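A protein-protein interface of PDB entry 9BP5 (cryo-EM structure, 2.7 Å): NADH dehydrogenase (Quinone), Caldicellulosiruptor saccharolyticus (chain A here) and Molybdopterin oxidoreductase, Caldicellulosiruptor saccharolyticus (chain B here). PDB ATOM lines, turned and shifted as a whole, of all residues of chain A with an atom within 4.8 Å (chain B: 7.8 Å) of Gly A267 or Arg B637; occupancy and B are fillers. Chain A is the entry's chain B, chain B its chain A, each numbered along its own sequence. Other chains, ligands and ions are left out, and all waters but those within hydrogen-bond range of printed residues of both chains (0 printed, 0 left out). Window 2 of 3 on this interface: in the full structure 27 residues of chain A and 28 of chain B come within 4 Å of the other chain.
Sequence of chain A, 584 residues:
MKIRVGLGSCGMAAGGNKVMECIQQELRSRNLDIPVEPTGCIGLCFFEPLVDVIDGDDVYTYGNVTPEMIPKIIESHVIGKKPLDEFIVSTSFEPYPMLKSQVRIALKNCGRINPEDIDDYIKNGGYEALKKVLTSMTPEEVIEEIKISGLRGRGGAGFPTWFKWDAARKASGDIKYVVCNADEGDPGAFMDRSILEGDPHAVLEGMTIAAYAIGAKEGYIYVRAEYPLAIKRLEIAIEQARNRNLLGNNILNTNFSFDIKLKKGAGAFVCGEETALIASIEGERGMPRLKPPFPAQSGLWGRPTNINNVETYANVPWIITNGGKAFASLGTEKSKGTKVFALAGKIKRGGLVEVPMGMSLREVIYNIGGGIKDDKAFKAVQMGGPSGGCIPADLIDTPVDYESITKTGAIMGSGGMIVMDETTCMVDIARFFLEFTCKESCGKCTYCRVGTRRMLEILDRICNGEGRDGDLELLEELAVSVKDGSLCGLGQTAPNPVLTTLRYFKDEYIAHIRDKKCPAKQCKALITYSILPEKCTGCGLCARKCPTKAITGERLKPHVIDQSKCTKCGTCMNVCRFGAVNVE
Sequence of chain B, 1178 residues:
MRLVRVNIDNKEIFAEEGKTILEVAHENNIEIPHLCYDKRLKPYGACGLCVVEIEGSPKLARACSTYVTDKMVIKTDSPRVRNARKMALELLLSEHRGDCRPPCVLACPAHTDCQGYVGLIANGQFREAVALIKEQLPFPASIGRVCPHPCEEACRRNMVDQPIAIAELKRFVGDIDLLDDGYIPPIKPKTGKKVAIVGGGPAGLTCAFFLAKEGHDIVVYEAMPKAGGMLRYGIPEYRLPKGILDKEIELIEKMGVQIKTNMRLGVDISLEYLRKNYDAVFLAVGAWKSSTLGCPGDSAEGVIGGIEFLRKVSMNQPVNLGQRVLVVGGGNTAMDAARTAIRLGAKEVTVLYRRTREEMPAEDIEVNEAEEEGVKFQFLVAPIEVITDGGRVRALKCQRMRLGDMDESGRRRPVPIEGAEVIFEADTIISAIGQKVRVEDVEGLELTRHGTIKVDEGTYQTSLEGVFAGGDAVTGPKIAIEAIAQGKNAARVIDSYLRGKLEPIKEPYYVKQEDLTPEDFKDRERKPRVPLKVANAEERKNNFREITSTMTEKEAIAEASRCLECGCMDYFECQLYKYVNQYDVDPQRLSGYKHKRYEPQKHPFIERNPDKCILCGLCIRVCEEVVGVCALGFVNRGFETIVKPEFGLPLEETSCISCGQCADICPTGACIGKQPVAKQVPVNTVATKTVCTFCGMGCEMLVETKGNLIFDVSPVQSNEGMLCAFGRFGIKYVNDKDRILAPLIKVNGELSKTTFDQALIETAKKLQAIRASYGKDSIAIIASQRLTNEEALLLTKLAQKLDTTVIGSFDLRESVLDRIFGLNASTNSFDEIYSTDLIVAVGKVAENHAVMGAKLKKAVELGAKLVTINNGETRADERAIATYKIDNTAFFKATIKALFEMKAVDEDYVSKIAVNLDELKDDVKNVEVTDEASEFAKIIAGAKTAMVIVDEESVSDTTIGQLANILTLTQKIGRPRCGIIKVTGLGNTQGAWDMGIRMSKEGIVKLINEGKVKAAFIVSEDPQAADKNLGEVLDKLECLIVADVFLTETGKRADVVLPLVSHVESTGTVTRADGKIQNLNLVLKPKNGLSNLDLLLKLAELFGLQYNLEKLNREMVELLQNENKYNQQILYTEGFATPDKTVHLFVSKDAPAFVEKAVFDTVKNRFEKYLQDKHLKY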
ATOM      1  N   ARG A 224       8.492   0.510  -7.867  1.00  0.00           N
ATOM      2  CA  ARG A 224       8.114   0.443  -9.269  1.00  0.00           C
ATOM      3  C   ARG A 224       7.361   1.701  -9.672  1.00  0.00           C
ATOM      4  O   ARG A 224       6.531   2.216  -8.921  1.00  0.00           O
ATOM      5  CB  ARG A 224       7.259  -0.791  -9.531  1.00  0.00           C
ATOM      6  CG  ARG A 224       7.913  -2.085  -9.117  1.00  0.00           C
ATOM      7  CD  ARG A 224       8.317  -2.883 -10.333  1.00  0.00           C
ATOM      8  NE  ARG A 224       7.173  -3.197 -11.177  1.00  0.00           N
ATOM      9  CZ  ARG A 224       6.657  -4.409 -11.317  1.00  0.00           C
ATOM     10  NH1 ARG A 224       7.161  -5.451 -10.678  1.00  0.00           N
ATOM     11  NH2 ARG A 224       5.613  -4.580 -12.121  1.00  0.00           N
ATOM     12  N   GLY A 265      11.640   2.015 -10.210  1.00  0.00           N
ATOM     13  CA  GLY A 265      11.916   0.856 -11.031  1.00  0.00           C
ATOM     14  C   GLY A 265      11.141   0.886 -12.335  1.00  0.00           C
ATOM     15  O   GLY A 265      10.011   1.361 -12.406  1.00  0.00           O
ATOM     16  N   ALA A 266      11.776   0.371 -13.387  1.00  0.00           N
ATOM     17  CA  ALA A 266      11.143   0.345 -14.698  1.00  0.00           C
ATOM     18  C   ALA A 266      10.176  -0.817 -14.863  1.00  0.00           C
ATOM     19  O   ALA A 266       9.356  -0.795 -15.783  1.00  0.00           O
ATOM     20  CB  ALA A 266      12.203   0.290 -15.796  1.00  0.00           C
ATOM     21  N   GLY A 267      10.247  -1.822 -13.998  1.00  0.00           N
ATOM     22  CA  GLY A 267       9.299  -2.915 -14.051  1.00  0.00           C
ATOM     23  C   GLY A 267       9.885  -4.224 -14.535  1.00  0.00           C
ATOM     24  O   GLY A 267      10.034  -4.439 -15.741  1.00  0.00           O
ATOM     25  N   ALA A 268      10.207  -5.111 -13.596  1.00  0.00           N
ATOM     26  CA  ALA A 268      10.705  -6.442 -13.915  1.00  0.00           C
ATOM     27  C   ALA A 268      10.668  -7.326 -12.677  1.00  0.00           C
ATOM     28  O   ALA A 268      11.114  -6.914 -11.603  1.00  0.00           O
ATOM     29  CB  ALA A 268      12.126  -6.370 -14.474  1.00  0.00           C
ATOM     30  N   PHE A 269      10.127  -8.538 -12.812  1.00  0.00           N
ATOM     31  CA  PHE A 269      10.138  -9.474 -11.693  1.00  0.00           C
ATOM     32  C   PHE A 269      11.558  -9.869 -11.322  1.00  0.00           C
ATOM     33  O   PHE A 269      11.844 -10.130 -10.149  1.00  0.00           O
ATOM     34  CB  PHE A 269       9.314 -10.712 -12.038  1.00  0.00           C
ATOM     35  CG  PHE A 269       9.113 -11.655 -10.889  1.00  0.00           C
ATOM     36  CD1 PHE A 269       8.475 -11.240  -9.740  1.00  0.00           C
ATOM     37  CD2 PHE A 269       9.547 -12.963 -10.967  1.00  0.00           C
ATOM     38  CE1 PHE A 269       8.282 -12.106  -8.687  1.00  0.00           C
ATOM     39  CE2 PHE A 269       9.357 -13.833  -9.916  1.00  0.00           C
ATOM     40  CZ  PHE A 269       8.724 -13.404  -8.775  1.00  0.00           C
ATOM     41  N   LYS A 439       7.500 -14.930 -19.123  1.00  0.00           N
ATOM     42  CA  LYS A 439       7.408 -13.550 -19.576  1.00  0.00           C
ATOM     43  C   LYS A 439       8.254 -12.594 -18.746  1.00  0.00           C
ATOM     44  O   LYS A 439       8.489 -11.465 -19.186  1.00  0.00           O
ATOM     45  CB  LYS A 439       5.946 -13.089 -19.584  1.00  0.00           C
ATOM     46  CG  LYS A 439       5.549 -12.180 -18.435  1.00  0.00           C
ATOM     47  CD  LYS A 439       4.066 -11.849 -18.489  1.00  0.00           C
ATOM     48  CE  LYS A 439       3.730 -10.661 -17.602  1.00  0.00           C
ATOM     49  NZ  LYS A 439       2.397 -10.803 -16.953  1.00  0.00           N
ATOM     50  N   GLU A 440       8.735 -13.014 -17.576  1.00  0.00           N
ATOM     51  CA  GLU A 440       9.525 -12.146 -16.710  1.00  0.00           C
ATOM     52  C   GLU A 440      10.933 -12.669 -16.459  1.00  0.00           C
ATOM     53  O   GLU A 440      11.643 -12.117 -15.613  1.00  0.00           O
ATOM     54  CB  GLU A 440       8.811 -11.928 -15.375  1.00  0.00           C
ATOM     55  CG  GLU A 440       7.519 -11.135 -15.492  1.00  0.00           C
ATOM     56  CD  GLU A 440       7.743  -9.633 -15.488  1.00  0.00           C
ATOM     57  OE1 GLU A 440       8.327  -9.114 -14.516  1.00  0.00           O
ATOM     58  OE2 GLU A 440       7.329  -8.965 -16.459  1.00  0.00           O
ATOM     59  N   SER A 441      11.358 -13.711 -17.162  1.00  0.00           N
ATOM     60  CA  SER A 441      12.713 -14.217 -17.013  1.00  0.00           C
ATOM     61  C   SER A 441      13.703 -13.314 -17.737  1.00  0.00           C
ATOM     62  O   SER A 441      13.406 -12.757 -18.795  1.00  0.00           O
ATOM     63  CB  SER A 441      12.813 -15.640 -17.555  1.00  0.00           C
ATOM     64  OG  SER A 441      14.102 -16.175 -17.322  1.00  0.00           O
ATOM     65  N   CYS A 442      14.897 -13.174 -17.155  1.00  0.00           N
ATOM     66  CA  CYS A 442      15.897 -12.296 -17.752  1.00  0.00           C
ATOM     67  C   CYS A 442      16.536 -12.909 -18.989  1.00  0.00           C
ATOM     68  O   CYS A 442      17.149 -12.181 -19.778  1.00  0.00           O
ATOM     69  CB  CYS A 442      16.982 -11.945 -16.738  1.00  0.00           C
ATOM     70  SG  CYS A 442      18.413 -13.023 -16.781  1.00  0.00           S
ATOM     71  N   ARG B 597      14.769 -15.851 -37.041  1.00  0.00           N
ATOM     72  CA  ARG B 597      15.014 -14.420 -37.155  1.00  0.00           C
ATOM     73  C   ARG B 597      16.255 -14.105 -37.979  1.00  0.00           C
ATOM     74  O   ARG B 597      16.771 -12.986 -37.911  1.00  0.00           O
ATOM     75  CB  ARG B 597      15.134 -13.789 -35.768  1.00  0.00           C
ATOM     76  CG  ARG B 597      14.126 -14.298 -34.770  1.00  0.00           C
ATOM     77  CD  ARG B 597      14.229 -13.554 -33.462  1.00  0.00           C
ATOM     78  NE  ARG B 597      15.102 -14.236 -32.516  1.00  0.00           N
ATOM     79  CZ  ARG B 597      15.240 -13.886 -31.245  1.00  0.00           C
ATOM     80  NH1 ARG B 597      14.576 -12.866 -30.734  1.00  0.00           N
ATOM     81  NH2 ARG B 597      16.068 -14.580 -30.471  1.00  0.00           N
ATOM     82  N   PHE B 634      22.300  -6.888 -25.903  1.00  0.00           N
ATOM     83  CA  PHE B 634      21.101  -7.705 -25.798  1.00  0.00           C
ATOM     84  C   PHE B 634      19.873  -6.875 -26.129  1.00  0.00           C
ATOM     85  O   PHE B 634      19.782  -5.703 -25.768  1.00  0.00           O
ATOM     86  CB  PHE B 634      20.965  -8.287 -24.393  1.00  0.00           C
ATOM     87  CG  PHE B 634      21.878  -9.438 -24.117  1.00  0.00           C
ATOM     88  CD1 PHE B 634      21.800 -10.595 -24.865  1.00  0.00           C
ATOM     89  CD2 PHE B 634      22.810  -9.367 -23.100  1.00  0.00           C
ATOM     90  CE1 PHE B 634      22.638 -11.657 -24.609  1.00  0.00           C
ATOM     91  CE2 PHE B 634      23.649 -10.425 -22.844  1.00  0.00           C
ATOM     92  CZ  PHE B 634      23.562 -11.572 -23.599  1.00  0.00           C
ATOM     93  N   VAL B 635      18.929  -7.489 -26.828  1.00  0.00           N
ATOM     94  CA  VAL B 635      17.662  -6.872 -27.181  1.00  0.00           C
ATOM     95  C   VAL B 635      16.556  -7.825 -26.754  1.00  0.00           C
ATOM     96  O   VAL B 635      16.725  -9.048 -26.777  1.00  0.00           O
ATOM     97  CB  VAL B 635      17.583  -6.549 -28.690  1.00  0.00           C
ATOM     98  CG1 VAL B 635      16.277  -5.866 -29.042  1.00  0.00           C
ATOM     99  CG2 VAL B 635      18.751  -5.679 -29.098  1.00  0.00           C
ATOM    100  N   ASN B 636      15.428  -7.249 -26.333  1.00  0.00           N
ATOM    101  CA  ASN B 636      14.282  -7.968 -25.788  1.00  0.00           C
ATOM    102  C   ASN B 636      14.642  -8.609 -24.457  1.00  0.00           C
ATOM    103  O   ASN B 636      15.658  -8.262 -23.851  1.00  0.00           O
ATOM    104  CB  ASN B 636      13.760  -9.021 -26.767  1.00  0.00           C
ATOM    105  CG  ASN B 636      13.418  -8.444 -28.113  1.00  0.00           C
ATOM    106  OD1 ASN B 636      12.908  -7.334 -28.210  1.00  0.00           O
ATOM    107  ND2 ASN B 636      13.697  -9.195 -29.164  1.00  0.00           N
ATOM    108  N   ARG B 637      13.814  -9.535 -23.988  1.00  0.00           N
ATOM    109  CA  ARG B 637      14.015 -10.107 -22.669  1.00  0.00           C
ATOM    110  C   ARG B 637      13.382 -11.489 -22.631  1.00  0.00           C
ATOM    111  O   ARG B 637      12.263 -11.675 -23.112  1.00  0.00           O
ATOM    112  CB  ARG B 637      13.416  -9.196 -21.591  1.00  0.00           C
ATOM    113  CG  ARG B 637      13.558  -9.697 -20.181  1.00  0.00           C
ATOM    114  CD  ARG B 637      12.236  -9.613 -19.448  1.00  0.00           C
ATOM    115  NE  ARG B 637      11.874  -8.241 -19.113  1.00  0.00           N
ATOM    116  CZ  ARG B 637      10.766  -7.897 -18.474  1.00  0.00           C
ATOM    117  NH1 ARG B 637       9.873  -8.799 -18.105  1.00  0.00           N
ATOM    118  NH2 ARG B 637      10.546  -6.615 -18.200  1.00  0.00           N
ATOM    119  N   GLY B 638      14.109 -12.449 -22.072  1.00  0.00           N
ATOM    120  CA  GLY B 638      13.595 -13.793 -21.898  1.00  0.00           C
ATOM    121  C   GLY B 638      13.811 -14.692 -23.091  1.00  0.00           C
ATOM    122  O   GLY B 638      14.911 -14.754 -23.644  1.00  0.00           O
ATOM    123  N   PHE B 639      12.761 -15.407 -23.490  1.00  0.00           N
ATOM    124  CA  PHE B 639      12.841 -16.246 -24.675  1.00  0.00           C
ATOM    125  C   PHE B 639      13.038 -15.428 -25.943  1.00  0.00           C
ATOM    126  O   PHE B 639      13.518 -15.966 -26.945  1.00  0.00           O
ATOM    127  CB  PHE B 639      11.582 -17.103 -24.791  1.00  0.00           C
ATOM    128  CG  PHE B 639      11.736 -18.286 -25.695  1.00  0.00           C
ATOM    129  CD1 PHE B 639      12.493 -19.372 -25.308  1.00  0.00           C
ATOM    130  CD2 PHE B 639      11.119 -18.312 -26.930  1.00  0.00           C
ATOM    131  CE1 PHE B 639      12.636 -20.457 -26.136  1.00  0.00           C
ATOM    132  CE2 PHE B 639      11.259 -19.396 -27.763  1.00  0.00           C
ATOM    133  CZ  PHE B 639      12.019 -20.468 -27.366  1.00  0.00           C
ATOM    134  N   GLU B 640      12.690 -14.146 -25.922  1.00  0.00           N
ATOM    135  CA  GLU B 640      12.821 -13.281 -27.085  1.00  0.00           C
ATOM    136  C   GLU B 640      14.174 -12.600 -27.169  1.00  0.00           C
ATOM    137  O   GLU B 640      14.389 -11.801 -28.082  1.00  0.00           O
ATOM    138  CB  GLU B 640      11.722 -12.218 -27.074  1.00  0.00           C
ATOM    139  CG  GLU B 640      10.343 -12.775 -26.830  1.00  0.00           C
ATOM    140  CD  GLU B 640       9.771 -13.448 -28.055  1.00  0.00           C
ATOM    141  OE1 GLU B 640      10.214 -13.117 -29.173  1.00  0.00           O
ATOM    142  OE2 GLU B 640       8.881 -14.309 -27.901  1.00  0.00           O
ATOM    143  N   THR B 641      15.083 -12.893 -26.244  1.00  0.00           N
ATOM    144  CA  THR B 641      16.368 -12.214 -26.214  1.00  0.00           C
ATOM    145  C   THR B 641      17.152 -12.506 -27.483  1.00  0.00           C
ATOM    146  O   THR B 641      17.228 -13.652 -27.933  1.00  0.00           O
ATOM    147  CB  THR B 641      17.168 -12.653 -24.989  1.00  0.00           C
ATOM    148  OG1 THR B 641      16.331 -12.605 -23.831  1.00  0.00           O
ATOM    149  CG2 THR B 641      18.344 -11.730 -24.773  1.00  0.00           C
ATOM    150  N   ILE B 642      17.731 -11.459 -28.062  1.00  0.00           N
ATOM    151  CA  ILE B 642      18.556 -11.571 -29.253  1.00  0.00           C
ATOM    152  C   ILE B 642      19.786 -10.701 -29.036  1.00  0.00           C
ATOM    153  O   ILE B 642      19.814  -9.840 -28.160  1.00  0.00           O
ATOM    154  CB  ILE B 642      17.773 -11.159 -30.525  1.00  0.00           C
ATOM    155  CG1 ILE B 642      18.448 -11.674 -31.796  1.00  0.00           C
ATOM    156  CG2 ILE B 642      17.565  -9.658 -30.578  1.00  0.00           C
ATOM    157  CD1 ILE B 642      17.640 -11.444 -33.034  1.00  0.00           C
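The guanidinium group of Arg B637 lies within hydrogen-bond range of the backbone carbonyl oxygen of Gly A267 (3.3 Å). The guanidinium group of Arg B637 sits at hydrogen-bond distance from the backbone carbonyl oxygen of Lys A439, 3.2 Å away. The side-chain carboxylate of Glu A440 is in salt-bridge range of the guanidinium group of Arg B637 (3.0 Å). N of Gly B638 lies close to O of Ser A441 (3.4 Å).
The backbone carbonyl oxygen (O) of Gly B638 is in hydrogen-bond range of the side-chain hydroxyl (OG1) of Thr B641, at 2.6 Å. N of Phe A269 is in hydrogen-bond range of OE1 of Glu A440 (2.5 Å).
Arg B637 touches Ser A441. O of Cys A442 touches N of Gly B638 (3.8 Å).
No residue of chain B comes within 4 Å of Ala A266. Of the printed residues of chain B, Lys A439 touches Arg B637. Printed residues of chain B within 4 Å of Glu A440: Arg B637. Of the printed residues of chain B, Cys A442 touches Gly B638 (3.8 Å). Glu B640 touches none of the printed residues of chain A. Thr B641 touches none of the printed residues of chain A. The nearest printed residue of chain B that does not touch Gly A267 is Asn B636 (10.6 Å). The nearest printed residue of chain B that does not touch Cys A442 is Thr B641 (4.2 Å).
Of the 10 printed residues of chain A, 5 touch a printed residue of chain B. Of the 10 printed residues of chain B, 2 touch a printed residue of chain A. Among the printed residues, 6 pairs touch across the chains. Among the printed residues, Asp or Glu carboxylates within 4 Å of a Lys or Arg side-chain nitrogen of the other chain: Glu A440 with Arg B637 (3.0 Å).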
